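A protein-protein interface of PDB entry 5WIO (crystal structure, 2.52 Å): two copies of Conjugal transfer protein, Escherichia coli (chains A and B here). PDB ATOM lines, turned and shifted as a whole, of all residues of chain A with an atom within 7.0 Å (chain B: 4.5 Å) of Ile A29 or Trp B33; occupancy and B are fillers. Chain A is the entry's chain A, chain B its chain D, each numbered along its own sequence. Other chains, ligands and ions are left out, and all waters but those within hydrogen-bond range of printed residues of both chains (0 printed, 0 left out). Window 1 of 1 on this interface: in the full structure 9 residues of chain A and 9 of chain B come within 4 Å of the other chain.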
ATOM      1  N   SER A  24      24.321  17.457  25.047  1.00  0.00           N
ATOM      2  CA  SER A  24      25.112  16.332  25.535  1.00  0.00           C
ATOM      3  C   SER A  24      24.269  15.305  26.283  1.00  0.00           C
ATOM      4  O   SER A  24      23.209  15.624  26.816  1.00  0.00           O
ATOM      5  CB  SER A  24      26.240  16.834  26.439  1.00  0.00           C
ATOM      6  OG  SER A  24      27.007  15.750  26.929  1.00  0.00           O
ATOM      7  N   TYR A  25      24.758  14.068  26.319  1.00  0.00           N
ATOM      8  CA  TYR A  25      24.057  12.977  26.986  1.00  0.00           C
ATOM      9  C   TYR A  25      24.954  12.235  27.977  1.00  0.00           C
ATOM     10  O   TYR A  25      24.601  11.157  28.455  1.00  0.00           O
ATOM     11  CB  TYR A  25      23.503  11.989  25.955  1.00  0.00           C
ATOM     12  CG  TYR A  25      22.021  12.128  25.680  1.00  0.00           C
ATOM     13  CD1 TYR A  25      21.087  11.431  26.436  1.00  0.00           C
ATOM     14  CD2 TYR A  25      21.557  12.947  24.659  1.00  0.00           C
ATOM     15  CE1 TYR A  25      19.732  11.549  26.187  1.00  0.00           C
ATOM     16  CE2 TYR A  25      20.203  13.071  24.401  1.00  0.00           C
ATOM     17  CZ  TYR A  25      19.296  12.370  25.170  1.00  0.00           C
ATOM     18  OH  TYR A  25      17.948  12.489  24.919  1.00  0.00           O
ATOM     19  N   GLY A  26      26.111  12.812  28.284  1.00  0.00           N
ATOM     20  CA  GLY A  26      27.055  12.188  29.196  1.00  0.00           C
ATOM     21  C   GLY A  26      28.294  11.680  28.484  1.00  0.00           C
ATOM     22  O   GLY A  26      28.327  11.612  27.257  1.00  0.00           O
ATOM     23  N   ASP A  27      29.315  11.316  29.255  1.00  0.00           N
ATOM     24  CA  ASP A  27      30.581  10.867  28.682  1.00  0.00           C
ATOM     25  C   ASP A  27      30.438   9.588  27.863  1.00  0.00           C
ATOM     26  O   ASP A  27      30.806   9.550  26.689  1.00  0.00           O
ATOM     27  CB  ASP A  27      31.623  10.649  29.785  1.00  0.00           C
ATOM     28  CG  ASP A  27      32.104  11.951  30.398  1.00  0.00           C
ATOM     29  OD1 ASP A  27      31.288  12.884  30.524  1.00  0.00           O
ATOM     30  OD2 ASP A  27      33.299  12.039  30.751  1.00  0.00           O
ATOM     31  N   GLU A  28      29.906   8.545  28.489  1.00  0.00           N
ATOM     32  CA  GLU A  28      29.814   7.231  27.859  1.00  0.00           C
ATOM     33  C   GLU A  28      28.915   7.244  26.626  1.00  0.00           C
ATOM     34  O   GLU A  28      29.256   6.666  25.593  1.00  0.00           O
ATOM     35  CB  GLU A  28      29.302   6.189  28.858  1.00  0.00           C
ATOM     36  CG  GLU A  28      30.202   5.981  30.068  1.00  0.00           C
ATOM     37  CD  GLU A  28      30.102   7.110  31.074  1.00  0.00           C
ATOM     38  OE1 GLU A  28      29.132   7.892  30.997  1.00  0.00           O
ATOM     39  OE2 GLU A  28      30.994   7.216  31.943  1.00  0.00           O
ATOM     40  N   ILE A  29      27.766   7.902  26.739  1.00  0.00           N
ATOM     41  CA  ILE A  29      26.813   7.970  25.635  1.00  0.00           C
ATOM     42  C   ILE A  29      27.398   8.708  24.438  1.00  0.00           C
ATOM     43  O   ILE A  29      27.395   8.192  23.321  1.00  0.00           O
ATOM     44  CB  ILE A  29      25.507   8.660  26.060  1.00  0.00           C
ATOM     45  CG1 ILE A  29      24.811   7.850  27.154  1.00  0.00           C
ATOM     46  CG2 ILE A  29      24.589   8.839  24.862  1.00  0.00           C
ATOM     47  CD1 ILE A  29      23.487   8.426  27.591  1.00  0.00           C
ATOM     48  N   ASP A  30      27.900   9.915  24.678  1.00  0.00           N
ATOM     49  CA  ASP A  30      28.484  10.723  23.614  1.00  0.00           C
ATOM     50  C   ASP A  30      29.664  10.009  22.965  1.00  0.00           C
ATOM     51  O   ASP A  30      29.830  10.045  21.746  1.00  0.00           O
ATOM     52  CB  ASP A  30      28.924  12.085  24.154  1.00  0.00           C
ATOM     53  CG  ASP A  30      27.762  12.908  24.677  1.00  0.00           C
ATOM     54  OD1 ASP A  30      26.606  12.590  24.328  1.00  0.00           O
ATOM     55  OD2 ASP A  30      28.003  13.872  25.433  1.00  0.00           O
ATOM     56  N   LYS A  31      30.470   9.351  23.793  1.00  0.00           N
ATOM     57  CA  LYS A  31      31.641   8.620  23.321  1.00  0.00           C
ATOM     58  C   LYS A  31      31.275   7.527  22.322  1.00  0.00           C
ATOM     59  O   LYS A  31      31.978   7.320  21.331  1.00  0.00           O
ATOM     60  CB  LYS A  31      32.392   8.004  24.501  1.00  0.00           C
ATOM     61  CG  LYS A  31      33.532   7.094  24.094  1.00  0.00           C
ATOM     62  CD  LYS A  31      34.117   6.370  25.294  1.00  0.00           C
ATOM     63  CE  LYS A  31      35.149   5.340  24.857  1.00  0.00           C
ATOM     64  NZ  LYS A  31      35.694   4.580  26.011  1.00  0.00           N
ATOM     65  N   PHE A  32      30.179   6.826  22.585  1.00  0.00           N
ATOM     66  CA  PHE A  32      29.752   5.738  21.712  1.00  0.00           C
ATOM     67  C   PHE A  32      29.293   6.257  20.353  1.00  0.00           C
ATOM     68  O   PHE A  32      29.685   5.725  19.315  1.00  0.00           O
ATOM     69  CB  PHE A  32      28.634   4.929  22.368  1.00  0.00           C
ATOM     70  CG  PHE A  32      27.956   3.971  21.435  1.00  0.00           C
ATOM     71  CD1 PHE A  32      28.539   2.754  21.125  1.00  0.00           C
ATOM     72  CD2 PHE A  32      26.737   4.290  20.863  1.00  0.00           C
ATOM     73  CE1 PHE A  32      27.919   1.871  20.264  1.00  0.00           C
ATOM     74  CE2 PHE A  32      26.111   3.412  20.002  1.00  0.00           C
ATOM     75  CZ  PHE A  32      26.702   2.202  19.701  1.00  0.00           C
ATOM     76  N   TRP A  33      28.462   7.294  20.365  1.00  0.00           N
ATOM     77  CA  TRP A  33      27.947   7.876  19.129  1.00  0.00           C
ATOM     78  C   TRP A  33      29.057   8.503  18.290  1.00  0.00           C
ATOM     79  O   TRP A  33      29.039   8.421  17.061  1.00  0.00           O
ATOM     80  CB  TRP A  33      26.872   8.924  19.433  1.00  0.00           C
ATOM     81  CG  TRP A  33      25.638   8.362  20.064  1.00  0.00           C
ATOM     82  CD1 TRP A  33      25.103   8.705  21.271  1.00  0.00           C
ATOM     83  CD2 TRP A  33      24.784   7.347  19.521  1.00  0.00           C
ATOM     84  NE1 TRP A  33      23.967   7.971  21.512  1.00  0.00           N
ATOM     85  CE2 TRP A  33      23.750   7.130  20.453  1.00  0.00           C
ATOM     86  CE3 TRP A  33      24.792   6.604  18.336  1.00  0.00           C
ATOM     87  CZ2 TRP A  33      22.736   6.202  20.237  1.00  0.00           C
ATOM     88  CZ3 TRP A  33      23.784   5.681  18.125  1.00  0.00           C
ATOM     89  CH2 TRP A  33      22.770   5.489  19.072  1.00  0.00           C
ATOM     90  N   LEU A  34      30.020   9.129  18.959  1.00  0.00           N
ATOM     91  CA  LEU A  34      31.121   9.796  18.272  1.00  0.00           C
ATOM     92  C   LEU A  34      32.048   8.798  17.584  1.00  0.00           C
ATOM     93  O   LEU A  34      32.441   8.996  16.434  1.00  0.00           O
ATOM     94  CB  LEU A  34      31.919  10.660  19.251  1.00  0.00           C
ATOM     95  CG  LEU A  34      31.194  11.875  19.832  1.00  0.00           C
ATOM     96  CD1 LEU A  34      32.062  12.566  20.870  1.00  0.00           C
ATOM     97  CD2 LEU A  34      30.806  12.843  18.727  1.00  0.00           C
ATOM     98  N   LEU A  97      36.220  14.682  25.308  1.00  0.00           N
ATOM     99  CA  LEU A  97      34.911  15.322  25.265  1.00  0.00           C
ATOM    100  C   LEU A  97      34.901  16.708  25.898  1.00  0.00           C
ATOM    101  O   LEU A  97      35.521  16.937  26.937  1.00  0.00           O
ATOM    102  CB  LEU A  97      33.866  14.446  25.960  1.00  0.00           C
ATOM    103  CG  LEU A  97      33.509  13.114  25.299  1.00  0.00           C
ATOM    104  CD1 LEU A  97      32.326  12.472  26.011  1.00  0.00           C
ATOM    105  CD2 LEU A  97      33.213  13.308  23.821  1.00  0.00           C
ATOM    106  N   TYR A 132      29.000  18.103  18.071  1.00  0.00           N
ATOM    107  CA  TYR A 132      27.835  17.225  18.068  1.00  0.00           C
ATOM    108  C   TYR A 132      26.688  17.759  18.918  1.00  0.00           C
ATOM    109  O   TYR A 132      26.872  18.643  19.755  1.00  0.00           O
ATOM    110  CB  TYR A 132      28.226  15.825  18.549  1.00  0.00           C
ATOM    111  CG  TYR A 132      28.642  15.755  20.001  1.00  0.00           C
ATOM    112  CD1 TYR A 132      29.923  16.116  20.397  1.00  0.00           C
ATOM    113  CD2 TYR A 132      27.754  15.318  20.977  1.00  0.00           C
ATOM    114  CE1 TYR A 132      30.309  16.048  21.724  1.00  0.00           C
ATOM    115  CE2 TYR A 132      28.130  15.249  22.306  1.00  0.00           C
ATOM    116  CZ  TYR A 132      29.409  15.614  22.673  1.00  0.00           C
ATOM    117  OH  TYR A 132      29.788  15.546  23.995  1.00  0.00           O
ATOM    118  N   TYR A 134      22.128  16.672  19.988  1.00  0.00           N
ATOM    119  CA  TYR A 134      20.992  15.764  19.873  1.00  0.00           C
ATOM    120  C   TYR A 134      19.724  16.544  19.542  1.00  0.00           C
ATOM    121  O   TYR A 134      19.138  17.190  20.410  1.00  0.00           O
ATOM    122  CB  TYR A 134      20.801  14.965  21.163  1.00  0.00           C
ATOM    123  CG  TYR A 134      21.969  14.073  21.515  1.00  0.00           C
ATOM    124  CD1 TYR A 134      23.106  14.591  22.122  1.00  0.00           C
ATOM    125  CD2 TYR A 134      21.933  12.712  21.243  1.00  0.00           C
ATOM    126  CE1 TYR A 134      24.174  13.778  22.446  1.00  0.00           C
ATOM    127  CE2 TYR A 134      22.996  11.892  21.564  1.00  0.00           C
ATOM    128  CZ  TYR A 134      24.114  12.429  22.165  1.00  0.00           C
ATOM    129  OH  TYR A 134      25.176  11.615  22.485  1.00  0.00           O
ATOM    130  N   LEU A 149      18.531   8.619  19.821  1.00  0.00           N
ATOM    131  CA  LEU A 149      18.619   9.900  20.519  1.00  0.00           C
ATOM    132  C   LEU A 149      18.771  11.082  19.567  1.00  0.00           C
ATOM    133  O   LEU A 149      18.906  12.223  20.007  1.00  0.00           O
ATOM    134  CB  LEU A 149      19.785   9.887  21.510  1.00  0.00           C
ATOM    135  CG  LEU A 149      19.603   9.034  22.767  1.00  0.00           C
ATOM    136  CD1 LEU A 149      20.854   9.072  23.632  1.00  0.00           C
ATOM    137  CD2 LEU A 149      18.388   9.506  23.557  1.00  0.00           C
ATOM    138  N   PHE A 151      21.251  11.789  17.514  1.00  0.00           N
ATOM    139  CA  PHE A 151      22.606  12.322  17.508  1.00  0.00           C
ATOM    140  C   PHE A 151      22.962  12.876  16.135  1.00  0.00           C
ATOM    141  O   PHE A 151      22.666  12.261  15.112  1.00  0.00           O
ATOM    142  CB  PHE A 151      23.608  11.240  17.917  1.00  0.00           C
ATOM    143  CG  PHE A 151      25.044  11.648  17.753  1.00  0.00           C
ATOM    144  CD1 PHE A 151      25.685  12.392  18.729  1.00  0.00           C
ATOM    145  CD2 PHE A 151      25.756  11.281  16.623  1.00  0.00           C
ATOM    146  CE1 PHE A 151      27.006  12.766  18.578  1.00  0.00           C
ATOM    147  CE2 PHE A 151      27.078  11.650  16.467  1.00  0.00           C
ATOM    148  CZ  PHE A 151      27.704  12.394  17.447  1.00  0.00           C
ATOM    149  N   ILE B  29      24.102  -0.657  19.308  1.00  0.00           N
ATOM    150  CA  ILE B  29      23.418   0.058  20.380  1.00  0.00           C
ATOM    151  C   ILE B  29      23.111  -0.876  21.546  1.00  0.00           C
ATOM    152  O   ILE B  29      23.168  -0.472  22.707  1.00  0.00           O
ATOM    153  CB  ILE B  29      22.115   0.710  19.887  1.00  0.00           C
ATOM    154  CG1 ILE B  29      22.423   1.770  18.828  1.00  0.00           C
ATOM    155  CG2 ILE B  29      21.360   1.331  21.051  1.00  0.00           C
ATOM    156  CD1 ILE B  29      21.207   2.537  18.359  1.00  0.00           C
ATOM    157  N   ASP B  30      22.797  -2.129  21.232  1.00  0.00           N
ATOM    158  CA  ASP B  30      22.529  -3.125  22.264  1.00  0.00           C
ATOM    159  C   ASP B  30      23.816  -3.552  22.962  1.00  0.00           C
ATOM    160  O   ASP B  30      23.862  -3.665  24.186  1.00  0.00           O
ATOM    161  CB  ASP B  30      21.826  -4.346  21.667  1.00  0.00           C
ATOM    162  CG  ASP B  30      20.402  -4.049  21.246  1.00  0.00           C
ATOM    163  OD1 ASP B  30      19.792  -3.126  21.824  1.00  0.00           O
ATOM    164  OD2 ASP B  30      19.891  -4.741  20.340  1.00  0.00           O
ATOM    165  N   LYS B  31      24.861  -3.784  22.173  1.00  0.00           N
ATOM    166  CA  LYS B  31      26.143  -4.232  22.705  1.00  0.00           C
ATOM    167  C   LYS B  31      26.758  -3.203  23.648  1.00  0.00           C
ATOM    168  O   LYS B  31      27.546  -3.548  24.527  1.00  0.00           O
ATOM    169  CB  LYS B  31      27.115  -4.537  21.564  1.00  0.00           C
ATOM    170  CG  LYS B  31      26.647  -5.637  20.630  1.00  0.00           C
ATOM    171  CD  LYS B  31      27.625  -5.840  19.489  1.00  0.00           C
ATOM    172  CE  LYS B  31      27.126  -6.890  18.512  1.00  0.00           C
ATOM    173  NZ  LYS B  31      28.066  -7.075  17.375  1.00  0.00           N
ATOM    174  N   PHE B  32      26.395  -1.938  23.460  1.00  0.00           N
ATOM    175  CA  PHE B  32      26.910  -0.868  24.305  1.00  0.00           C
ATOM    176  C   PHE B  32      26.371  -0.983  25.725  1.00  0.00           C
ATOM    177  O   PHE B  32      27.137  -1.029  26.685  1.00  0.00           O
ATOM    178  CB  PHE B  32      26.562   0.500  23.716  1.00  0.00           C
ATOM    179  CG  PHE B  32      27.060   1.657  24.537  1.00  0.00           C
ATOM    180  CD1 PHE B  32      28.394   2.023  24.503  1.00  0.00           C
ATOM    181  CD2 PHE B  32      26.192   2.380  25.336  1.00  0.00           C
ATOM    182  CE1 PHE B  32      28.854   3.088  25.256  1.00  0.00           C
ATOM    183  CE2 PHE B  32      26.644   3.445  26.089  1.00  0.00           C
ATOM    184  CZ  PHE B  32      27.978   3.800  26.049  1.00  0.00           C
ATOM    185  N   TRP B  33      25.048  -1.034  25.854  1.00  0.00           N
ATOM    186  CA  TRP B  33      24.414  -1.132  27.162  1.00  0.00           C
ATOM    187  C   TRP B  33      24.762  -2.448  27.851  1.00  0.00           C
ATOM    188  O   TRP B  33      24.870  -2.507  29.075  1.00  0.00           O
ATOM    189  CB  TRP B  33      22.895  -0.993  27.038  1.00  0.00           C
ATOM    190  CG  TRP B  33      22.462   0.271  26.369  1.00  0.00           C
ATOM    191  CD1 TRP B  33      21.727   0.382  25.226  1.00  0.00           C
ATOM    192  CD2 TRP B  33      22.749   1.607  26.795  1.00  0.00           C
ATOM    193  NE1 TRP B  33      21.531   1.706  24.916  1.00  0.00           N
ATOM    194  CE2 TRP B  33      22.149   2.479  25.864  1.00  0.00           C
ATOM    195  CE3 TRP B  33      23.451   2.153  27.873  1.00  0.00           C
ATOM    196  CZ2 TRP B  33      22.231   3.865  25.979  1.00  0.00           C
ATOM    197  CZ3 TRP B  33      23.531   3.528  27.985  1.00  0.00           C
ATOM    198  CH2 TRP B  33      22.924   4.369  27.045  1.00  0.00           C
ATOM    199  N   LEU B  34      24.937  -3.498  27.057  1.00  0.00           N
ATOM    200  CA  LEU B  34      25.281  -4.812  27.590  1.00  0.00           C
ATOM    201  C   LEU B  34      26.673  -4.810  28.210  1.00  0.00           C
ATOM    202  O   LEU B  34      26.839  -5.138  29.386  1.00  0.00           O
ATOM    203  CB  LEU B  34      25.196  -5.876  26.493  1.00  0.00           C
ATOM    204  CG  LEU B  34      23.807  -6.144  25.914  1.00  0.00           C
ATOM    205  CD1 LEU B  34      23.883  -7.181  24.804  1.00  0.00           C
ATOM    206  CD2 LEU B  34      22.849  -6.592  27.006  1.00  0.00           C
ATOM    207  N   THR B  35      27.669  -4.441  27.411  1.00  0.00           N
ATOM    208  CA  THR B  35      29.049  -4.389  27.880  1.00  0.00           C
ATOM    209  C   THR B  35      29.192  -3.401  29.033  1.00  0.00           C
ATOM    210  O   THR B  35      29.895  -3.669  30.007  1.00  0.00           O
ATOM    211  CB  THR B  35      30.018  -3.996  26.749  1.00  0.00           C
ATOM    212  OG1 THR B  35      29.653  -2.712  26.227  1.00  0.00           O
ATOM    213  CG2 THR B  35      29.971  -5.025  25.631  1.00  0.00           C
ATOM    214  N   GLN B  36      28.517  -2.261  28.917  1.00  0.00           N
ATOM    215  CA  GLN B  36      28.515  -1.266  29.981  1.00  0.00           C
ATOM    216  C   GLN B  36      27.896  -1.836  31.253  1.00  0.00           C
ATOM    217  O   GLN B  36      28.330  -1.519  32.360  1.00  0.00           O
ATOM    218  CB  GLN B  36      27.760  -0.008  29.543  1.00  0.00           C
ATOM    219  CG  GLN B  36      28.502   0.837  28.518  1.00  0.00           C
ATOM    220  CD  GLN B  36      29.737   1.501  29.096  1.00  0.00           C
ATOM    221  OE1 GLN B  36      29.713   2.009  30.217  1.00  0.00           O
ATOM    222  NE2 GLN B  36      30.825   1.497  28.334  1.00  0.00           N
ATOM    223  N   TYR B  37      26.887  -2.685  31.087  1.00  0.00           N
ATOM    224  CA  TYR B  37      26.215  -3.304  32.226  1.00  0.00           C
ATOM    225  C   TYR B  37      27.131  -4.303  32.924  1.00  0.00           C
ATOM    226  O   TYR B  37      27.205  -4.338  34.152  1.00  0.00           O
ATOM    227  CB  TYR B  37      24.925  -3.998  31.783  1.00  0.00           C
ATOM    228  CG  TYR B  37      24.061  -4.456  32.935  1.00  0.00           C
ATOM    229  CD1 TYR B  37      24.280  -5.683  33.549  1.00  0.00           C
ATOM    230  CD2 TYR B  37      23.032  -3.657  33.415  1.00  0.00           C
ATOM    231  CE1 TYR B  37      23.493  -6.103  34.603  1.00  0.00           C
ATOM    232  CE2 TYR B  37      22.241  -4.068  34.469  1.00  0.00           C
ATOM    233  CZ  TYR B  37      22.476  -5.293  35.060  1.00  0.00           C
ATOM    234  OH  TYR B  37      21.689  -5.706  36.111  1.00  0.00           O
ATOM    235  N   MET B  59      19.295   0.118  34.980  1.00  0.00           N
ATOM    236  CA  MET B  59      19.398  -0.813  33.861  1.00  0.00           C
ATOM    237  C   MET B  59      18.922  -2.211  34.237  1.00  0.00           C
ATOM    238  O   MET B  59      19.131  -3.168  33.491  1.00  0.00           O
ATOM    239  CB  MET B  59      20.841  -0.880  33.355  1.00  0.00           C
ATOM    240  CG  MET B  59      21.398   0.443  32.857  1.00  0.00           C
ATOM    241  SD  MET B  59      23.088   0.282  32.248  1.00  0.00           S
ATOM    242  CE  MET B  59      23.427   1.963  31.735  1.00  0.00           C
ATOM    243  N   TYR B 134      13.486  -3.154  26.067  1.00  0.00           N
ATOM    244  CA  TYR B 134      13.347  -1.716  25.877  1.00  0.00           C
ATOM    245  C   TYR B 134      11.931  -1.259  26.206  1.00  0.00           C
ATOM    246  O   TYR B 134      11.068  -1.199  25.332  1.00  0.00           O
ATOM    247  CB  TYR B 134      13.712  -1.323  24.444  1.00  0.00           C
ATOM    248  CG  TYR B 134      15.198  -1.346  24.164  1.00  0.00           C
ATOM    249  CD1 TYR B 134      15.822  -2.500  23.711  1.00  0.00           C
ATOM    250  CD2 TYR B 134      15.976  -0.211  24.356  1.00  0.00           C
ATOM    251  CE1 TYR B 134      17.181  -2.524  23.455  1.00  0.00           C
ATOM    252  CE2 TYR B 134      17.333  -0.225  24.103  1.00  0.00           C
ATOM    253  CZ  TYR B 134      17.930  -1.383  23.653  1.00  0.00           C
ATOM    254  OH  TYR B 134      19.282  -1.402  23.401  1.00  0.00           O
ATOM    255  N   ARG B 144      18.744  10.267  32.094  1.00  0.00           N
ATOM    256  CA  ARG B 144      19.340  10.778  30.864  1.00  0.00           C
ATOM    257  C   ARG B 144      20.856  10.494  30.769  1.00  0.00           C
ATOM    258  O   ARG B 144      21.339  10.111  29.704  1.00  0.00           O
ATOM    259  CB  ARG B 144      19.078  12.280  30.727  1.00  0.00           C
ATOM    260  CG  ARG B 144      17.686  12.709  31.160  1.00  0.00           C
ATOM    261  CD  ARG B 144      16.765  12.884  29.963  1.00  0.00           C
ATOM    262  NE  ARG B 144      15.388  13.151  30.366  1.00  0.00           N
ATOM    263  CZ  ARG B 144      14.994  14.252  30.999  1.00  0.00           C
ATOM    264  NH1 ARG B 144      13.720  14.410  31.328  1.00  0.00           N
ATOM    265  NH2 ARG B 144      15.875  15.194  31.303  1.00  0.00           N
ATOM    266  N   TYR B 145      21.600  10.672  31.860  1.00  0.00           N
ATOM    267  CA  TYR B 145      23.050  10.397  31.871  1.00  0.00           C
ATOM    268  C   TYR B 145      23.498   8.929  31.680  1.00  0.00           C
ATOM    269  O   TYR B 145      24.452   8.648  30.955  1.00  0.00           O
ATOM    270  CB  TYR B 145      23.682  10.964  33.146  1.00  0.00           C
ATOM    271  N   VAL B 146      22.797   8.016  32.346  1.00  0.00           N
ATOM    272  CA  VAL B 146      23.084   6.578  32.379  1.00  0.00           C
ATOM    273  C   VAL B 146      22.233   5.718  31.439  1.00  0.00           C
ATOM    274  O   VAL B 146      22.728   4.784  30.808  1.00  0.00           O
ATOM    275  CB  VAL B 146      22.957   6.017  33.809  1.00  0.00           C
ATOM    276  N   PRO B 148      18.867   6.761  29.122  1.00  0.00           N
ATOM    277  CA  PRO B 148      17.748   7.514  28.548  1.00  0.00           C
ATOM    278  C   PRO B 148      16.957   6.710  27.518  1.00  0.00           C
ATOM    279  O   PRO B 148      15.886   7.144  27.092  1.00  0.00           O
ATOM    280  CB  PRO B 148      18.441   8.704  27.886  1.00  0.00           C
ATOM    281  CG  PRO B 148      19.755   8.152  27.458  1.00  0.00           C
ATOM    282  CD  PRO B 148      20.152   7.135  28.504  1.00  0.00           C
ATOM    283  N   LEU B 149      17.483   5.556  27.118  1.00  0.00           N
ATOM    284  CA  LEU B 149      16.807   4.710  26.141  1.00  0.00           C
ATOM    285  C   LEU B 149      16.034   3.584  26.820  1.00  0.00           C
ATOM    286  O   LEU B 149      15.455   2.725  26.152  1.00  0.00           O
ATOM    287  CB  LEU B 149      17.810   4.133  25.142  1.00  0.00           C
ATOM    288  N   PHE B 151      17.092   1.034  28.753  1.00  0.00           N
ATOM    289  CA  PHE B 151      17.685  -0.298  28.707  1.00  0.00           C
ATOM    290  C   PHE B 151      17.541  -0.976  30.064  1.00  0.00           C
ATOM    291  O   PHE B 151      18.075  -0.499  31.066  1.00  0.00           O
ATOM    292  CB  PHE B 151      19.157  -0.226  28.300  1.00  0.00           C
ATOM    293  CG  PHE B 151      19.838  -1.565  28.255  1.00  0.00           C
ATOM    294  CD1 PHE B 151      19.818  -2.327  27.099  1.00  0.00           C
ATOM    295  CD2 PHE B 151      20.501  -2.060  29.366  1.00  0.00           C
ATOM    296  CE1 PHE B 151      20.443  -3.557  27.052  1.00  0.00           C
ATOM    297  CE2 PHE B 151      21.128  -3.290  29.325  1.00  0.00           C
ATOM    298  CZ  PHE B 151      21.100  -4.039  28.166  1.00  0.00           C
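The backbone NH (N) of Tyr A25 lies within hydrogen-bond range of the side-chain carboxylate (OD1) of Asp A30. The side-chain hydroxyl of Thr B35 lies within hydrogen-bond range of the backbone carbonyl oxygen of Phe B32 (3.1 Å).
Ile A29 touches Trp B33, and with the chains exchanged Trp A33 touches Ile B29. Phe A32 touches Ile B29, but with the chains exchanged Ile A29 does not touch Phe B32 (4.2 Å). Phe B32 touches its own counterpart, Phe A32. Of the 11 pairs that touch across the chains among the printed residues, 3 have their exchanged pair printed and touching as well.
Arg B144 touches Tyr A25 (O to CD1, 3.5 Å). Tyr A25 touches Tyr B145. Phe B32 touches Glu A28 (CZ to O, 3.2 Å). Ile A29 touches Trp B33 (CG1 to CH2, 3.96 Å). O of Arg B144 touches CD1 of Ile A29, at 3.5 Å. Ile A29 touches Tyr B145 (CD1 to O, 3.5 Å). Pro B148 touches Ile A29 (CD to CD1, 3.7 Å). Ile B29 touches Phe A32. CB of Phe A32 touches CE1 of Phe B32, at 3.4 Å. CH2 of Trp A33 touches CD1 of Ile B29, at 3.4 Å.
Trp B33 touches just one residue of chain A: Ile A29 (3.96 Å). Printed residues of chain B within 4 Å of Trp A33: Ile B29. Of the printed residues of chain A, Arg B144 touches Tyr A25 (3.5 Å) and Ile A29 (3.5 Å). Of the printed residues of chain B, Phe A32 touches Ile B29 (3.9 Å) and Phe B32 (3.4 Å). Of the printed residues of chain A, Ile B29 touches Phe A32 (3.9 Å) and Trp A33 (3.4 Å). Leu B34 touches none of the printed residues of chain A. The nearest residue of chain A that does not touch Trp B33 is Leu A149 (5.9 Å).
Of the 17 printed residues of chain B, 6 touch a printed residue of chain A. Of the 16 printed residues of chain A, 5 touch a printed residue of chain B. Hydrophobic or aromatic side chains of chain A within 4 Å of the printed part of chain B: Tyr A25, Ile A29, Phe A32 and Trp A33.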
